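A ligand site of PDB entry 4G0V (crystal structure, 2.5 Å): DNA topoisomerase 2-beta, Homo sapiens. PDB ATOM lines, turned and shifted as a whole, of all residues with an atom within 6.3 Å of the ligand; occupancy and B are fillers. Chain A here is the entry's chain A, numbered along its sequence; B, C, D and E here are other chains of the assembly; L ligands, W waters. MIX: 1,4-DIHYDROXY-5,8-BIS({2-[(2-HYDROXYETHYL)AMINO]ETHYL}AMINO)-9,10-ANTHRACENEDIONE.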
ATOM      1  N   LEU A  84      23.481   3.510  38.475  1.00  0.00           N
ATOM      2  CA  LEU A  84      24.245   4.357  37.562  1.00  0.00           C
ATOM      3  C   LEU A  84      23.815   4.051  36.123  1.00  0.00           C
ATOM      4  O   LEU A  84      23.684   2.884  35.744  1.00  0.00           O
ATOM      5  CB  LEU A  84      25.734   4.106  37.705  1.00  0.00           C
ATOM      6  CG  LEU A  84      26.311   4.308  39.104  1.00  0.00           C
ATOM      7  CD1 LEU A  84      27.777   3.941  39.122  1.00  0.00           C
ATOM      8  CD2 LEU A  84      26.107   5.744  39.538  1.00  0.00           C
ATOM      9  N   ARG A  85      23.594   5.103  35.344  1.00  0.00           N
ATOM     10  CA  ARG A  85      23.215   4.929  33.939  1.00  0.00           C
ATOM     11  C   ARG A  85      24.294   5.426  32.995  1.00  0.00           C
ATOM     12  O   ARG A  85      24.529   6.629  32.888  1.00  0.00           O
ATOM     13  CB  ARG A  85      21.905   5.653  33.644  1.00  0.00           C
ATOM     14  CG  ARG A  85      20.719   4.712  33.511  1.00  0.00           C
ATOM     15  CD  ARG A  85      19.434   5.490  33.564  1.00  0.00           C
ATOM     16  NE  ARG A  85      19.359   6.460  32.488  1.00  0.00           N
ATOM     17  CZ  ARG A  85      18.606   7.569  32.509  1.00  0.00           C
ATOM     18  NH1 ARG A  85      17.855   7.852  33.575  1.00  0.00           N
ATOM     19  NH2 ARG A  85      18.609   8.367  31.454  1.00  0.00           N
ATOM     20  N   GLY A  86      24.940   4.504  32.293  1.00  0.00           N
ATOM     21  CA  GLY A  86      25.975   4.861  31.335  1.00  0.00           C
ATOM     22  C   GLY A  86      27.363   4.886  31.955  1.00  0.00           C
ATOM     23  O   GLY A  86      27.497   4.977  33.176  1.00  0.00           O
ATOM     24  N   LYS A  87      28.389   4.804  31.108  1.00  0.00           N
ATOM     25  CA  LYS A  87      29.782   4.904  31.555  1.00  0.00           C
ATOM     26  C   LYS A  87      30.001   6.185  32.373  1.00  0.00           C
ATOM     27  O   LYS A  87      29.429   7.238  32.065  1.00  0.00           O
ATOM     28  CB  LYS A  87      30.734   4.874  30.346  1.00  0.00           C
ATOM     29  CG  LYS A  87      30.553   3.637  29.433  1.00  0.00           C
ATOM     30  CD  LYS A  87      30.831   2.337  30.195  1.00  0.00           C
ATOM     31  CE  LYS A  87      30.603   1.080  29.359  1.00  0.00           C
ATOM     32  NZ  LYS A  87      31.717   0.832  28.420  1.00  0.00           N
ATOM     33  N   ILE A  88      30.799   6.085  33.441  1.00  0.00           N
ATOM     34  CA  ILE A  88      31.069   7.256  34.255  1.00  0.00           C
ATOM     35  C   ILE A  88      32.395   7.911  33.901  1.00  0.00           C
ATOM     36  O   ILE A  88      33.230   7.344  33.196  1.00  0.00           O
ATOM     37  CB  ILE A  88      31.056   6.959  35.780  1.00  0.00           C
ATOM     38  CG1 ILE A  88      32.292   6.173  36.195  1.00  0.00           C
ATOM     39  CG2 ILE A  88      29.775   6.247  36.189  1.00  0.00           C
ATOM     40  CD1 ILE A  88      32.422   6.010  37.686  1.00  0.00           C
ATOM     41  N   LEU A  89      32.553   9.138  34.371  1.00  0.00           N
ATOM     42  CA  LEU A  89      33.757   9.927  34.149  1.00  0.00           C
ATOM     43  C   LEU A  89      35.009   9.209  34.675  1.00  0.00           C
ATOM     44  O   LEU A  89      35.035   8.776  35.818  1.00  0.00           O
ATOM     45  CB  LEU A  89      33.584  11.261  34.863  1.00  0.00           C
ATOM     46  CG  LEU A  89      34.671  12.316  34.819  1.00  0.00           C
ATOM     47  CD1 LEU A  89      34.779  12.878  33.428  1.00  0.00           C
ATOM     48  CD2 LEU A  89      34.340  13.400  35.838  1.00  0.00           C
ATOM     49  N   ASN A 102      29.975  16.631  37.388  1.00  0.00           N
ATOM     50  CA  ASN A 102      29.453  15.296  37.150  1.00  0.00           C
ATOM     51  C   ASN A 102      28.380  14.877  38.149  1.00  0.00           C
ATOM     52  O   ASN A 102      28.643  14.724  39.343  1.00  0.00           O
ATOM     53  CB  ASN A 102      30.558  14.245  37.105  1.00  0.00           C
ATOM     54  CG  ASN A 102      30.026  12.870  36.714  1.00  0.00           C
ATOM     55  OD1 ASN A 102      29.732  12.037  37.562  1.00  0.00           O
ATOM     56  ND2 ASN A 102      29.881  12.644  35.417  1.00  0.00           N
ATOM     57  N   ALA A 103      27.174  14.658  37.634  1.00  0.00           N
ATOM     58  CA  ALA A 103      26.054  14.225  38.450  1.00  0.00           C
ATOM     59  C   ALA A 103      26.332  12.925  39.213  1.00  0.00           C
ATOM     60  O   ALA A 103      26.015  12.826  40.400  1.00  0.00           O
ATOM     61  CB  ALA A 103      24.830  14.058  37.586  1.00  0.00           C
ATOM     62  N   GLU A 104      26.911  11.951  38.533  1.00  0.00           N
ATOM     63  CA  GLU A 104      27.073  10.622  39.115  1.00  0.00           C
ATOM     64  C   GLU A 104      28.095  10.573  40.234  1.00  0.00           C
ATOM     65  O   GLU A 104      27.849   9.992  41.284  1.00  0.00           O
ATOM     66  CB  GLU A 104      27.431   9.600  38.031  1.00  0.00           C
ATOM     67  CG  GLU A 104      26.235   9.014  37.307  1.00  0.00           C
ATOM     68  CD  GLU A 104      25.817   9.841  36.115  1.00  0.00           C
ATOM     69  OE1 GLU A 104      26.596  10.727  35.697  1.00  0.00           O
ATOM     70  OE2 GLU A 104      24.700   9.599  35.605  1.00  0.00           O
ATOM     71  N   ILE A 105      29.254  11.168  40.005  1.00  0.00           N
ATOM     72  CA  ILE A 105      30.301  11.174  41.013  1.00  0.00           C
ATOM     73  C   ILE A 105      29.816  11.913  42.252  1.00  0.00           C
ATOM     74  O   ILE A 105      29.962  11.405  43.368  1.00  0.00           O
ATOM     75  CB  ILE A 105      31.590  11.773  40.440  1.00  0.00           C
ATOM     76  CG1 ILE A 105      32.438  10.652  39.865  1.00  0.00           C
ATOM     77  CG2 ILE A 105      32.379  12.486  41.508  1.00  0.00           C
ATOM     78  CD1 ILE A 105      32.803  10.873  38.439  1.00  0.00           C
ATOM     79  N   GLY A 358      22.512  -2.340  22.943  1.00  0.00           N
ATOM     80  CA  GLY A 358      21.435  -1.388  22.824  1.00  0.00           C
ATOM     81  C   GLY A 358      21.288  -1.014  21.369  1.00  0.00           C
ATOM     82  O   GLY A 358      22.261  -0.984  20.620  1.00  0.00           O
ATOM     83  N   GLN A 360      20.058   1.764  19.909  1.00  0.00           N
ATOM     84  CA  GLN A 360      20.286   3.142  19.466  1.00  0.00           C
ATOM     85  C   GLN A 360      21.666   3.242  18.792  1.00  0.00           C
ATOM     86  O   GLN A 360      21.847   3.987  17.832  1.00  0.00           O
ATOM     87  CB  GLN A 360      20.131   4.151  20.626  1.00  0.00           C
ATOM     88  CG  GLN A 360      20.062   5.637  20.215  1.00  0.00           C
ATOM     89  CD  GLN A 360      20.026   6.577  21.419  1.00  0.00           C
ATOM     90  OE1 GLN A 360      18.964   7.069  21.815  1.00  0.00           O
ATOM     91  NE2 GLN A 360      21.200   6.825  22.012  1.00  0.00           N
ATOM     92  N   ALA A 361      22.617   2.476  19.311  1.00  0.00           N
ATOM     93  CA  ALA A 361      23.928   2.414  18.698  1.00  0.00           C
ATOM     94  C   ALA A 361      23.795   1.928  17.255  1.00  0.00           C
ATOM     95  O   ALA A 361      24.353   2.546  16.349  1.00  0.00           O
ATOM     96  CB  ALA A 361      24.851   1.508  19.492  1.00  0.00           C
ATOM     97  N   MET A 364      22.289   4.488  14.983  1.00  0.00           N
ATOM     98  CA  MET A 364      23.274   5.492  14.634  1.00  0.00           C
ATOM     99  C   MET A 364      24.250   4.971  13.582  1.00  0.00           C
ATOM    100  O   MET A 364      24.609   5.697  12.654  1.00  0.00           O
ATOM    101  CB  MET A 364      23.992   6.033  15.872  1.00  0.00           C
ATOM    102  CG  MET A 364      23.109   6.974  16.701  1.00  0.00           C
ATOM    103  SD  MET A 364      23.823   7.379  18.337  1.00  0.00           S
ATOM    104  CE  MET A 364      25.309   8.299  17.890  1.00  0.00           C
ATOM    105  P    DT B   1      18.826   0.013  25.818  1.00  0.00           P
ATOM    106  OP1  DT B   1      17.815   0.460  24.843  1.00  0.00           O
ATOM    107  OP2  DT B   1      20.269   0.174  25.538  1.00  0.00           O
ATOM    108  O5'  DT B   1      18.489   0.723  27.214  1.00  0.00           O
ATOM    109  C5'  DT B   1      19.024   0.239  28.420  1.00  0.00           C
ATOM    110  C4'  DT B   1      19.155   1.390  29.378  1.00  0.00           C
ATOM    111  O4'  DT B   1      20.054   2.408  28.859  1.00  0.00           O
ATOM    112  C3'  DT B   1      17.845   2.122  29.631  1.00  0.00           C
ATOM    113  O3'  DT B   1      17.095   1.396  30.594  1.00  0.00           O
ATOM    114  C2'  DT B   1      18.370   3.449  30.164  1.00  0.00           C
ATOM    115  C1'  DT B   1      19.614   3.682  29.292  1.00  0.00           C
ATOM    116  N1   DT B   1      19.303   4.551  28.121  1.00  0.00           N
ATOM    117  C2   DT B   1      19.287   5.904  28.348  1.00  0.00           C
ATOM    118  O2   DT B   1      19.523   6.390  29.444  1.00  0.00           O
ATOM    119  N3   DT B   1      18.988   6.687  27.247  1.00  0.00           N
ATOM    120  C4   DT B   1      18.692   6.220  25.984  1.00  0.00           C
ATOM    121  O4   DT B   1      18.425   6.974  25.056  1.00  0.00           O
ATOM    122  C5   DT B   1      18.707   4.785  25.819  1.00  0.00           C
ATOM    123  C7   DT B   1      18.398   4.220  24.458  1.00  0.00           C
ATOM    124  C6   DT B   1      18.999   4.022  26.884  1.00  0.00           C
ATOM    125  P    DA C   4      19.653  18.193  25.694  1.00  0.00           P
ATOM    126  OP1  DA C   4      20.146  19.563  25.962  1.00  0.00           O
ATOM    127  OP2  DA C   4      19.953  17.527  24.403  1.00  0.00           O
ATOM    128  O5'  DA C   4      20.152  17.250  26.876  1.00  0.00           O
ATOM    129  C5'  DA C   4      19.983  17.649  28.225  1.00  0.00           C
ATOM    130  C4'  DA C   4      20.520  16.554  29.143  1.00  0.00           C
ATOM    131  O4'  DA C   4      19.586  15.441  29.160  1.00  0.00           O
ATOM    132  C3'  DA C   4      21.868  15.963  28.735  1.00  0.00           C
ATOM    133  O3'  DA C   4      22.892  16.680  29.417  1.00  0.00           O
ATOM    134  C2'  DA C   4      21.794  14.526  29.229  1.00  0.00           C
ATOM    135  C1'  DA C   4      20.297  14.221  29.202  1.00  0.00           C
ATOM    136  N9   DA C   4      19.874  13.397  28.069  1.00  0.00           N
ATOM    137  C8   DA C   4      19.595  13.823  26.795  1.00  0.00           C
ATOM    138  N7   DA C   4      19.249  12.839  25.998  1.00  0.00           N
ATOM    139  C5   DA C   4      19.284  11.717  26.800  1.00  0.00           C
ATOM    140  C6   DA C   4      19.010  10.348  26.554  1.00  0.00           C
ATOM    141  N6   DA C   4      18.623   9.873  25.365  1.00  0.00           N
ATOM    142  N1   DA C   4      19.163   9.482  27.573  1.00  0.00           N
ATOM    143  C2   DA C   4      19.536   9.954  28.761  1.00  0.00           C
ATOM    144  N3   DA C   4      19.828  11.211  29.120  1.00  0.00           N
ATOM    145  C4   DA C   4      19.668  12.044  28.073  1.00  0.00           C
ATOM    146  P    DG C   5      24.383  16.740  28.839  1.00  0.00           P
ATOM    147  OP1  DG C   5      25.081  17.828  29.558  1.00  0.00           O
ATOM    148  OP2  DG C   5      24.386  16.704  27.358  1.00  0.00           O
ATOM    149  O5'  DG C   5      25.002  15.347  29.289  1.00  0.00           O
ATOM    150  C5'  DG C   5      25.063  14.987  30.652  1.00  0.00           C
ATOM    151  C4'  DG C   5      26.193  13.993  30.799  1.00  0.00           C
ATOM    152  O4'  DG C   5      25.908  12.798  30.031  1.00  0.00           O
ATOM    153  C3'  DG C   5      27.577  14.454  30.344  1.00  0.00           C
ATOM    154  O3'  DG C   5      28.472  13.818  31.213  1.00  0.00           O
ATOM    155  C2'  DG C   5      27.696  13.871  28.944  1.00  0.00           C
ATOM    156  C1'  DG C   5      27.009  12.527  29.191  1.00  0.00           C
ATOM    157  N9   DG C   5      26.554  11.821  27.990  1.00  0.00           N
ATOM    158  C8   DG C   5      26.107  12.373  26.813  1.00  0.00           C
ATOM    159  N7   DG C   5      25.772  11.482  25.911  1.00  0.00           N
ATOM    160  C5   DG C   5      26.022  10.261  26.531  1.00  0.00           C
ATOM    161  C6   DG C   5      25.857   8.934  26.055  1.00  0.00           C
ATOM    162  O6   DG C   5      25.447   8.518  24.956  1.00  0.00           O
ATOM    163  N1   DG C   5      26.234   7.994  27.005  1.00  0.00           N
ATOM    164  C2   DG C   5      26.701   8.305  28.262  1.00  0.00           C
ATOM    165  N2   DG C   5      27.008   7.254  29.040  1.00  0.00           N
ATOM    166  N3   DG C   5      26.859   9.538  28.724  1.00  0.00           N
ATOM    167  C4   DG C   5      26.503  10.466  27.803  1.00  0.00           C
ATOM    168  P    DC C   6      29.857  14.515  31.645  1.00  0.00           P
ATOM    169  OP1  DC C   6      29.831  14.513  33.121  1.00  0.00           O
ATOM    170  OP2  DC C   6      30.033  15.790  30.903  1.00  0.00           O
ATOM    171  O5'  DC C   6      30.975  13.528  31.047  1.00  0.00           O
ATOM    172  C5'  DC C   6      31.382  12.343  31.720  1.00  0.00           C
ATOM    173  C4'  DC C   6      31.401  11.030  30.922  1.00  0.00           C
ATOM    174  O4'  DC C   6      30.260  10.847  30.042  1.00  0.00           O
ATOM    175  C3'  DC C   6      32.553  10.664  29.986  1.00  0.00           C
ATOM    176  O3'  DC C   6      33.716  10.465  30.723  1.00  0.00           O
ATOM    177  C2'  DC C   6      31.992   9.311  29.563  1.00  0.00           C
ATOM    178  C1'  DC C   6      30.498   9.609  29.408  1.00  0.00           C
ATOM    179  N1   DC C   6      30.003   9.673  27.985  1.00  0.00           N
ATOM    180  C2   DC C   6      29.810   8.470  27.313  1.00  0.00           C
ATOM    181  O2   DC C   6      30.082   7.431  27.904  1.00  0.00           O
ATOM    182  N3   DC C   6      29.344   8.472  26.047  1.00  0.00           N
ATOM    183  C4   DC C   6      29.073   9.618  25.442  1.00  0.00           C
ATOM    184  N4   DC C   6      28.616   9.554  24.187  1.00  0.00           N
ATOM    185  C5   DC C   6      29.261  10.867  26.102  1.00  0.00           C
ATOM    186  C6   DC C   6      29.723  10.849  27.354  1.00  0.00           C
ATOM    187  P    DG D   7      28.896  -1.660  18.611  1.00  0.00           P
ATOM    188  OP1  DG D   7      29.472  -2.883  18.022  1.00  0.00           O
ATOM    189  OP2  DG D   7      27.613  -1.152  18.103  1.00  0.00           O
ATOM    190  O5'  DG D   7      28.770  -1.890  20.183  1.00  0.00           O
ATOM    191  C5'  DG D   7      27.858  -1.138  20.983  1.00  0.00           C
ATOM    192  C4'  DG D   7      28.504  -0.821  22.320  1.00  0.00           C
ATOM    193  O4'  DG D   7      29.378   0.322  22.199  1.00  0.00           O
ATOM    194  C3'  DG D   7      27.560  -0.491  23.470  1.00  0.00           C
ATOM    195  O3'  DG D   7      27.226  -1.698  24.117  1.00  0.00           O
ATOM    196  C2'  DG D   7      28.433   0.349  24.368  1.00  0.00           C
ATOM    197  C1'  DG D   7      29.287   1.110  23.379  1.00  0.00           C
ATOM    198  N9   DG D   7      28.754   2.423  23.043  1.00  0.00           N
ATOM    199  C8   DG D   7      27.950   2.772  21.991  1.00  0.00           C
ATOM    200  N7   DG D   7      27.645   4.042  21.969  1.00  0.00           N
ATOM    201  C5   DG D   7      28.283   4.578  23.072  1.00  0.00           C
ATOM    202  C6   DG D   7      28.326   5.899  23.559  1.00  0.00           C
ATOM    203  O6   DG D   7      27.777   6.900  23.075  1.00  0.00           O
ATOM    204  N1   DG D   7      29.094   6.003  24.724  1.00  0.00           N
ATOM    205  C2   DG D   7      29.755   4.948  25.318  1.00  0.00           C
ATOM    206  N2   DG D   7      30.471   5.214  26.425  1.00  0.00           N
ATOM    207  N3   DG D   7      29.722   3.691  24.859  1.00  0.00           N
ATOM    208  C4   DG D   7      28.972   3.580  23.741  1.00  0.00           C
ATOM    209  P    DC D   8      25.873  -1.805  24.981  1.00  0.00           P
ATOM    210  OP1  DC D   8      25.724  -3.216  25.394  1.00  0.00           O
ATOM    211  OP2  DC D   8      24.790  -1.176  24.216  1.00  0.00           O
ATOM    212  O5'  DC D   8      26.184  -0.880  26.255  1.00  0.00           O
ATOM    213  C5'  DC D   8      27.167  -1.265  27.205  1.00  0.00           C
ATOM    214  C4'  DC D   8      27.243  -0.249  28.327  1.00  0.00           C
ATOM    215  O4'  DC D   8      27.625   1.047  27.808  1.00  0.00           O
ATOM    216  C3'  DC D   8      25.924  -0.054  29.080  1.00  0.00           C
ATOM    217  O3'  DC D   8      26.164  -0.010  30.469  1.00  0.00           O
ATOM    218  C2'  DC D   8      25.414   1.293  28.601  1.00  0.00           C
ATOM    219  C1'  DC D   8      26.690   2.025  28.210  1.00  0.00           C
ATOM    220  N1   DC D   8      26.309   2.969  27.144  1.00  0.00           N
ATOM    221  C2   DC D   8      26.491   4.331  27.387  1.00  0.00           C
ATOM    222  O2   DC D   8      27.024   4.703  28.457  1.00  0.00           O
ATOM    223  N3   DC D   8      26.100   5.222  26.434  1.00  0.00           N
ATOM    224  C4   DC D   8      25.521   4.803  25.298  1.00  0.00           C
ATOM    225  N4   DC D   8      25.167   5.752  24.408  1.00  0.00           N
ATOM    226  C5   DC D   8      25.330   3.418  25.036  1.00  0.00           C
ATOM    227  C6   DC D   8      25.719   2.544  25.990  1.00  0.00           C
ATOM    228  N   TYR E 403      13.350  -4.547  25.649  1.00  0.00           N
ATOM    229  CA  TYR E 403      13.905  -5.551  26.554  1.00  0.00           C
ATOM    230  C   TYR E 403      12.860  -6.580  26.961  1.00  0.00           C
ATOM    231  O   TYR E 403      13.072  -7.354  27.899  1.00  0.00           O
ATOM    232  CB  TYR E 403      14.534  -4.861  27.750  1.00  0.00           C
ATOM    233  CG  TYR E 403      15.671  -3.976  27.335  1.00  0.00           C
ATOM    234  CD1 TYR E 403      16.933  -4.519  27.102  1.00  0.00           C
ATOM    235  CD2 TYR E 403      15.493  -2.618  27.122  1.00  0.00           C
ATOM    236  CE1 TYR E 403      17.982  -3.728  26.687  1.00  0.00           C
ATOM    237  CE2 TYR E 403      16.546  -1.804  26.713  1.00  0.00           C
ATOM    238  CZ  TYR E 403      17.794  -2.368  26.501  1.00  0.00           C
ATOM    239  OH  TYR E 403      18.865  -1.587  26.091  1.00  0.00           O
HETATM  240  OAC MIX L   1      23.924   7.895  21.664  1.00  0.00           O
HETATM  241  CAK MIX L   1      23.611   8.968  22.580  1.00  0.00           C
HETATM  242  CAM MIX L   1      24.329  10.275  22.208  1.00  0.00           C
HETATM  243  NAS MIX L   1      23.980  11.336  23.141  1.00  0.00           N
HETATM  244  CAO MIX L   1      22.577  11.600  23.442  1.00  0.00           C
HETATM  245  CAQ MIX L   1      22.218  11.416  24.914  1.00  0.00           C
HETATM  246  NAU MIX L   1      22.114  10.034  25.338  1.00  0.00           N
HETATM  247  CAY MIX L   1      22.453   9.725  26.633  1.00  0.00           C
HETATM  248  CAI MIX L   1      22.705  10.763  27.532  1.00  0.00           C
HETATM  249  CAJ MIX L   1      23.049  10.518  28.842  1.00  0.00           C
HETATM  250  CBE MIX L   1      22.554   8.405  27.080  1.00  0.00           C
HETATM  251  CBA MIX L   1      22.304   7.335  26.219  1.00  0.00           C
HETATM  252  OAA MIX L   1      21.997   7.539  25.031  1.00  0.00           O
HETATM  253  CBC MIX L   1      22.405   6.015  26.665  1.00  0.00           C
HETATM  254  CAW MIX L   1      22.154   4.957  25.790  1.00  0.00           C
HETATM  255  OAE MIX L   1      21.792   5.209  24.512  1.00  0.00           O
HETATM  256  CAG MIX L   1      22.263   3.640  26.225  1.00  0.00           C
HETATM  257  CAH MIX L   1      22.607   3.382  27.550  1.00  0.00           C
HETATM  258  CAX MIX L   1      22.858   4.446  28.418  1.00  0.00           C
HETATM  259  OAF MIX L   1      23.203   4.197  29.712  1.00  0.00           O
HETATM  260  CBD MIX L   1      22.749   5.764  27.983  1.00  0.00           C
HETATM  261  CBB MIX L   1      22.999   6.828  28.851  1.00  0.00           C
HETATM  262  OAB MIX L   1      23.314   6.613  30.043  1.00  0.00           O
HETATM  263  CBF MIX L   1      22.898   8.147  28.405  1.00  0.00           C
HETATM  264  CAZ MIX L   1      23.156   9.205  29.294  1.00  0.00           C
HETATM  265  NAV MIX L   1      23.499   8.973  30.589  1.00  0.00           N
HETATM  266  CAR MIX L   1      23.807  10.065  31.493  1.00  0.00           C
HETATM  267  CAP MIX L   1      24.913   9.701  32.472  1.00  0.00           C
HETATM  268  NAT MIX L   1      26.217  10.227  32.086  1.00  0.00           N
HETATM  269  CAN MIX L   1      27.431   9.522  32.467  1.00  0.00           C
HETATM  270  CAL MIX L   1      28.498  10.492  33.010  1.00  0.00           C
HETATM  271  OAD MIX L   1      28.929  10.111  34.346  1.00  0.00           O
HETATM  272  O   HOH W   1      21.949   1.721  31.414  1.00  0.00           O
HETATM  273  O   HOH W   2      26.460   8.036  21.064  1.00  0.00           O
HETATM  274  O   HOH W   3      25.112  14.354  23.793  1.00  0.00           O
HETATM  275  O   HOH W   4      23.155  14.703  25.657  1.00  0.00           O
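NAT of the ligand lies within salt-bridge range of OE1 of Glu 104 (3.7 Å).
ND2 of Asn 102 sits at hydrogen-bond distance from OAD of the ligand, at 2.9 Å.
An oxygen (OAC) of the ligand is in hydrogen-bond range of the side-chain amide nitrogen (NE2) of Gln 360, at 2.9 Å.
O4' of DG 5 of chain C lies within hydrogen-bond range of a nitrogen (NAT) of the ligand (3.3 Å).
N7 of DG 5 of chain C sits at hydrogen-bond distance from a nitrogen (NAS) of the ligand, 3.3 Å away.
O of Arg 85 sits close to NAV of the ligand (3.4 Å).
N of Gly 86 is in hydrogen-bond range of OAF of the ligand.
N4 of DC 8 of chain D sits close to OAE of the ligand, 3.4 Å away.
N6 of DA 4 of chain C lies close to a nitrogen (NAU) of the ligand (3.5 Å).
The side-chain sulfur (SD) of Met 364 lies within hydrogen-bond range of an oxygen (OAC) of the ligand (3.4 Å).
The side-chain amide oxygen (OD1) of Asn 102 sits at hydrogen-bond distance from the backbone NH (N) of Glu 104, 3.0 Å away.
OP1 of DC 6 of chain C is in hydrogen-bond range of ND2 of Asn 102, 3.0 Å away.
N of Ile 105 sits at hydrogen-bond distance from OD1 of Asn 102 (2.6 Å).
OE1 of Gln 360 lies close to O4 of DT 1 of chain B, at 3.3 Å.
P of DT 1 of chain B is covalently linked to the side-chain hydroxyl (OH) of Tyr 403 of chain E (1.6 Å).
O2 of DC 8 of chain D lies within hydrogen-bond range of N of Lys 87 (3.0 Å).
OP2 of DC 8 of chain D is in hydrogen-bond range of the backbone NH of Gly 358 (2.9 Å).
O2 of DC 6 of chain C lies close to N2 of DG 7 of chain D (2.7 Å).
Residues that only touch the ligand: Lys 87 (3.1 Å), Ile 88 (3.6 Å), Leu 89 (3.8 Å), DT 1 of chain B (3.0 Å) and DC 6 of chain C (3.5 Å).
Of the 21 residues printed, 14 come within 4 Å of the ligand.
The nearest printed residue that does not touch the ligand is DG 7 of chain D (4.2 Å).
Water W2 bridges an oxygen (OAC) of the ligand (2.6 Å) and O6 of DG 7 of chain D (2.7 Å).
Water W1 lies within hydrogen-bond range of O4' of DT 1 of chain B (3.3 Å) and OAF of the ligand (3.3 Å).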
